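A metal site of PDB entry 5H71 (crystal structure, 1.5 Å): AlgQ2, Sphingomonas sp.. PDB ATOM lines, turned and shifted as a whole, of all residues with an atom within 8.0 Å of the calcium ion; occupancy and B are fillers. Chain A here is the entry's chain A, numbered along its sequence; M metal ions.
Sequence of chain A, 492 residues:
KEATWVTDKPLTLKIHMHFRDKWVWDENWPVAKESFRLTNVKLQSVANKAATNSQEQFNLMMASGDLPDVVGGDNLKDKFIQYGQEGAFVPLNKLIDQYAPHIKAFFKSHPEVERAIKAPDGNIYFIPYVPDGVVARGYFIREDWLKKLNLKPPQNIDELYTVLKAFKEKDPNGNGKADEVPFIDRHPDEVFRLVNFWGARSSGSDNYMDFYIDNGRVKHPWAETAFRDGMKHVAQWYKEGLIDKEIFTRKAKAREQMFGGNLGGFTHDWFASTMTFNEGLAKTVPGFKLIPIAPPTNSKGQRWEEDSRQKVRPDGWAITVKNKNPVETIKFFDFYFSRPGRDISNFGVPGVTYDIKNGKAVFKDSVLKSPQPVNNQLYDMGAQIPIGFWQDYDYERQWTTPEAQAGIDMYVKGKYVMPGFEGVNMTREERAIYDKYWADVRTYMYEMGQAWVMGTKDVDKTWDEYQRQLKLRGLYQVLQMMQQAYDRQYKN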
ATOM      1  N   TRP A 145      33.997   6.145  33.757  1.00  0.00           N
ATOM      2  CA  TRP A 145      32.919   6.889  33.119  1.00  0.00           C
ATOM      3  C   TRP A 145      32.131   7.718  34.139  1.00  0.00           C
ATOM      4  O   TRP A 145      31.753   8.848  33.849  1.00  0.00           O
ATOM      5  CB  TRP A 145      31.979   5.943  32.358  1.00  0.00           C
ATOM      6  CG  TRP A 145      32.517   5.484  31.022  1.00  0.00           C
ATOM      7  CD1 TRP A 145      33.769   5.727  30.504  1.00  0.00           C
ATOM      8  CD2 TRP A 145      31.823   4.706  30.041  1.00  0.00           C
ATOM      9  NE1 TRP A 145      33.878   5.144  29.250  1.00  0.00           N
ATOM     10  CE2 TRP A 145      32.703   4.515  28.950  1.00  0.00           C
ATOM     11  CE3 TRP A 145      30.540   4.160  29.981  1.00  0.00           C
ATOM     12  CZ2 TRP A 145      32.336   3.799  27.815  1.00  0.00           C
ATOM     13  CZ3 TRP A 145      30.182   3.447  28.846  1.00  0.00           C
ATOM     14  CH2 TRP A 145      31.069   3.274  27.787  1.00  0.00           C
ATOM     15  N   PHE A 167      25.341   7.526  30.482  1.00  0.00           N
ATOM     16  CA  PHE A 167      26.263   6.744  29.670  1.00  0.00           C
ATOM     17  C   PHE A 167      25.840   6.745  28.200  1.00  0.00           C
ATOM     18  O   PHE A 167      26.656   6.867  27.294  1.00  0.00           O
ATOM     19  CB  PHE A 167      26.340   5.282  30.159  1.00  0.00           C
ATOM     20  CG  PHE A 167      27.089   5.082  31.459  1.00  0.00           C
ATOM     21  CD1 PHE A 167      27.754   6.115  32.099  1.00  0.00           C
ATOM     22  CD2 PHE A 167      27.114   3.811  32.027  1.00  0.00           C
ATOM     23  CE1 PHE A 167      28.431   5.891  33.295  1.00  0.00           C
ATOM     24  CE2 PHE A 167      27.806   3.564  33.207  1.00  0.00           C
ATOM     25  CZ  PHE A 167      28.470   4.605  33.852  1.00  0.00           C
ATOM     26  N   LYS A 168      24.544   6.560  27.983  1.00  0.00           N
ATOM     27  CA  LYS A 168      23.988   6.545  26.633  1.00  0.00           C
ATOM     28  C   LYS A 168      24.165   7.871  25.884  1.00  0.00           C
ATOM     29  O   LYS A 168      24.526   7.895  24.707  1.00  0.00           O
ATOM     30  CB  LYS A 168      22.495   6.215  26.696  1.00  0.00           C
ATOM     31  CG  LYS A 168      21.810   6.088  25.332  1.00  0.00           C
ATOM     32  CD  LYS A 168      22.138   4.766  24.670  1.00  0.00           C
ATOM     33  CE  LYS A 168      21.497   4.665  23.277  1.00  0.00           C
ATOM     34  NZ  LYS A 168      22.160   5.580  22.292  1.00  0.00           N
ATOM     35  N   GLU A 169      23.913   8.969  26.593  1.00  0.00           N
ATOM     36  CA  GLU A 169      23.685  10.249  25.940  1.00  0.00           C
ATOM     37  C   GLU A 169      24.873  11.197  25.985  1.00  0.00           C
ATOM     38  O   GLU A 169      24.967  12.121  25.168  1.00  0.00           O
ATOM     39  CB  GLU A 169      22.468  10.932  26.579  1.00  0.00           C
ATOM     40  CG  GLU A 169      21.133  10.269  26.221  1.00  0.00           C
ATOM     41  CD  GLU A 169      19.969  10.811  27.038  1.00  0.00           C
ATOM     42  OE1 GLU A 169      18.823  10.412  26.755  1.00  0.00           O
ATOM     43  OE2 GLU A 169      20.191  11.650  27.932  1.00  0.00           O
ATOM     44  N   LYS A 170      25.771  10.980  26.946  1.00  0.00           N
ATOM     45  CA  LYS A 170      26.803  11.987  27.215  1.00  0.00           C
ATOM     46  C   LYS A 170      28.218  11.601  26.761  1.00  0.00           C
ATOM     47  O   LYS A 170      29.202  12.196  27.193  1.00  0.00           O
ATOM     48  CB  LYS A 170      26.810  12.310  28.710  1.00  0.00           C
ATOM     49  CG  LYS A 170      25.524  13.014  29.129  1.00  0.00           C
ATOM     50  CD  LYS A 170      25.523  13.449  30.572  1.00  0.00           C
ATOM     51  CE  LYS A 170      24.838  14.803  30.716  1.00  0.00           C
ATOM     52  NZ  LYS A 170      23.367  14.744  30.485  1.00  0.00           N
ATOM     53  N   ASP A 171      28.302  10.638  25.845  1.00  0.00           N
ATOM     54  CA  ASP A 171      29.536  10.303  25.140  1.00  0.00           C
ATOM     55  C   ASP A 171      30.768  10.099  26.035  1.00  0.00           C
ATOM     56  O   ASP A 171      31.818  10.692  25.794  1.00  0.00           O
ATOM     57  CB  ASP A 171      29.853  11.412  24.107  1.00  0.00           C
ATOM     58  CG  ASP A 171      30.986  11.051  23.152  1.00  0.00           C
ATOM     59  OD1 ASP A 171      31.169   9.858  22.820  1.00  0.00           O
ATOM     60  OD2 ASP A 171      31.732  11.974  22.745  1.00  0.00           O
ATOM     61  N   PRO A 172      30.650   9.235  27.062  1.00  0.00           N
ATOM     62  CA  PRO A 172      31.815   9.094  27.946  1.00  0.00           C
ATOM     63  C   PRO A 172      33.075   8.529  27.284  1.00  0.00           C
ATOM     64  O   PRO A 172      34.151   8.769  27.850  1.00  0.00           O
ATOM     65  CB  PRO A 172      31.312   8.136  29.040  1.00  0.00           C
ATOM     66  CG  PRO A 172      30.163   7.404  28.402  1.00  0.00           C
ATOM     67  CD  PRO A 172      29.509   8.433  27.528  1.00  0.00           C
ATOM     68  N   ASN A 173      32.995   7.820  26.157  1.00  0.00           N
ATOM     69  CA  ASN A 173      34.236   7.348  25.549  1.00  0.00           C
ATOM     70  C   ASN A 173      34.832   8.433  24.635  1.00  0.00           C
ATOM     71  O   ASN A 173      35.913   8.252  24.055  1.00  0.00           O
ATOM     72  CB  ASN A 173      34.064   5.991  24.812  1.00  0.00           C
ATOM     73  CG  ASN A 173      33.212   6.068  23.544  1.00  0.00           C
ATOM     74  OD1 ASN A 173      32.949   7.135  23.001  1.00  0.00           O
ATOM     75  ND2 ASN A 173      32.787   4.888  23.079  1.00  0.00           N
ATOM     76  N   GLY A 174      34.126   9.558  24.519  1.00  0.00           N
ATOM     77  CA  GLY A 174      34.676  10.793  23.973  1.00  0.00           C
ATOM     78  C   GLY A 174      34.905  10.861  22.476  1.00  0.00           C
ATOM     79  O   GLY A 174      35.703  11.684  22.015  1.00  0.00           O
ATOM     80  N   ASN A 175      34.193  10.038  21.705  1.00  0.00           N
ATOM     81  CA  ASN A 175      34.435  10.018  20.261  1.00  0.00           C
ATOM     82  C   ASN A 175      33.374  10.781  19.457  1.00  0.00           C
ATOM     83  O   ASN A 175      33.398  10.780  18.225  1.00  0.00           O
ATOM     84  CB  ASN A 175      34.525   8.566  19.757  1.00  0.00           C
ATOM     85  CG  ASN A 175      33.252   7.742  19.993  1.00  0.00           C
ATOM     86  OD1 ASN A 175      32.211   8.271  20.375  1.00  0.00           O
ATOM     87  ND2 ASN A 175      33.364   6.442  19.778  1.00  0.00           N
ATOM     88  N   GLY A 176      32.471  11.455  20.159  1.00  0.00           N
ATOM     89  CA  GLY A 176      31.417  12.228  19.520  1.00  0.00           C
ATOM     90  C   GLY A 176      30.353  11.391  18.831  1.00  0.00           C
ATOM     91  O   GLY A 176      29.549  11.900  18.047  1.00  0.00           O
ATOM     92  N   LYS A 177      30.328  10.100  19.155  1.00  0.00           N
ATOM     93  CA  LYS A 177      29.343   9.180  18.613  1.00  0.00           C
ATOM     94  C   LYS A 177      28.473   8.644  19.742  1.00  0.00           C
ATOM     95  O   LYS A 177      28.938   8.426  20.854  1.00  0.00           O
ATOM     96  CB  LYS A 177      30.025   8.034  17.855  1.00  0.00           C
ATOM     97  CG  LYS A 177      30.767   8.473  16.605  1.00  0.00           C
ATOM     98  CD  LYS A 177      31.859   7.503  16.190  1.00  0.00           C
ATOM     99  CE  LYS A 177      31.391   6.074  16.093  1.00  0.00           C
ATOM    100  NZ  LYS A 177      32.468   5.186  15.576  1.00  0.00           N
ATOM    101  N   ALA A 178      27.187   8.443  19.456  1.00  0.00           N
ATOM    102  CA  ALA A 178      26.295   7.789  20.397  1.00  0.00           C
ATOM    103  C   ALA A 178      26.416   6.283  20.216  1.00  0.00           C
ATOM    104  O   ALA A 178      25.494   5.628  19.728  1.00  0.00           O
ATOM    105  CB  ALA A 178      24.867   8.249  20.200  1.00  0.00           C
ATOM    106  N   ASP A 179      27.566   5.737  20.603  1.00  0.00           N
ATOM    107  CA  ASP A 179      27.862   4.321  20.428  1.00  0.00           C
ATOM    108  C   ASP A 179      27.876   3.584  21.766  1.00  0.00           C
ATOM    109  O   ASP A 179      27.971   2.371  21.798  1.00  0.00           O
ATOM    110  CB  ASP A 179      29.191   4.141  19.675  1.00  0.00           C
ATOM    111  CG  ASP A 179      30.382   4.757  20.404  1.00  0.00           C
ATOM    112  OD1 ASP A 179      30.190   5.639  21.260  1.00  0.00           O
ATOM    113  OD2 ASP A 179      31.542   4.357  20.105  1.00  0.00           O
ATOM    114  N   GLU A 180      27.780   4.336  22.857  1.00  0.00           N
ATOM    115  CA  GLU A 180      27.767   3.708  24.179  1.00  0.00           C
ATOM    116  C   GLU A 180      26.560   2.807  24.349  1.00  0.00           C
ATOM    117  O   GLU A 180      25.444   3.171  23.984  1.00  0.00           O
ATOM    118  CB  GLU A 180      27.771   4.773  25.274  1.00  0.00           C
ATOM    119  CG  GLU A 180      29.145   5.454  25.495  1.00  0.00           C
ATOM    120  CD  GLU A 180      29.484   6.562  24.491  1.00  0.00           C
ATOM    121  OE1 GLU A 180      30.595   7.106  24.594  1.00  0.00           O
ATOM    122  OE2 GLU A 180      28.666   6.890  23.610  1.00  0.00           O
ATOM    123  N   VAL A 181      26.789   1.638  24.935  1.00  0.00           N
ATOM    124  CA  VAL A 181      25.737   0.674  25.226  1.00  0.00           C
ATOM    125  C   VAL A 181      25.755   0.437  26.735  1.00  0.00           C
ATOM    126  O   VAL A 181      26.630  -0.264  27.250  1.00  0.00           O
ATOM    127  CB  VAL A 181      25.975  -0.633  24.486  1.00  0.00           C
ATOM    128  CG1 VAL A 181      24.880  -1.615  24.833  1.00  0.00           C
ATOM    129  CG2 VAL A 181      26.061  -0.404  22.965  1.00  0.00           C
ATOM    130  N   ASN A 262      35.419  -0.411  24.390  1.00  0.00           N
ATOM    131  CA  ASN A 262      35.031   0.791  25.135  1.00  0.00           C
ATOM    132  C   ASN A 262      33.612   1.270  24.809  1.00  0.00           C
ATOM    133  O   ASN A 262      33.385   2.488  24.642  1.00  0.00           O
ATOM    134  CB  ASN A 262      36.023   1.931  24.905  1.00  0.00           C
ATOM    135  CG  ASN A 262      36.002   2.937  26.030  1.00  0.00           C
ATOM    136  OD1 ASN A 262      35.421   2.686  27.076  1.00  0.00           O
ATOM    137  ND2 ASN A 262      36.629   4.101  25.813  1.00  0.00           N
ATOM    138  N   LEU A 263      32.679   0.329  24.743  1.00  0.00           N
ATOM    139  CA  LEU A 263      31.267   0.624  24.511  1.00  0.00           C
ATOM    140  C   LEU A 263      30.374   0.389  25.740  1.00  0.00           C
ATOM    141  O   LEU A 263      29.356   1.074  25.925  1.00  0.00           O
ATOM    142  CB  LEU A 263      30.715  -0.226  23.360  1.00  0.00           C
ATOM    143  CG  LEU A 263      31.466  -0.106  22.036  1.00  0.00           C
ATOM    144  CD1 LEU A 263      30.811  -0.980  20.972  1.00  0.00           C
ATOM    145  CD2 LEU A 263      31.560   1.339  21.576  1.00  0.00           C
HETATM  146 CA    CA M   1      30.761   7.710  22.224  1.00  0.00          CA
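The calcium ion is bound by the side-chain carboxylate (OD1) of Asp 171, the side-chain carboxylate (OD1) of Asp 179, the backbone carbonyl oxygen (O) of Lys 177, the side-chain amide oxygen (OD1) of Asn 173, the side-chain amide oxygen (OD1) of Asn 175, the side-chain carboxylate (OE1) of Glu 180 and the side-chain carboxylate (OE2) of Glu 180. The calcium ion has seven donor atoms within binding distance.
The backbone NH (N) of Gly 174 sits close to the side-chain carboxylate (OD1) of Asp 171, at 3.4 Å. The backbone NH (N) of Gly 176 sits at hydrogen-bond distance from the side-chain carboxylate (OD2) of Asp 171, at 2.7 Å. The side-chain amide nitrogen of Asn 173 lies within hydrogen-bond range of the backbone carbonyl oxygen of Asn 262, 2.9 Å away.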
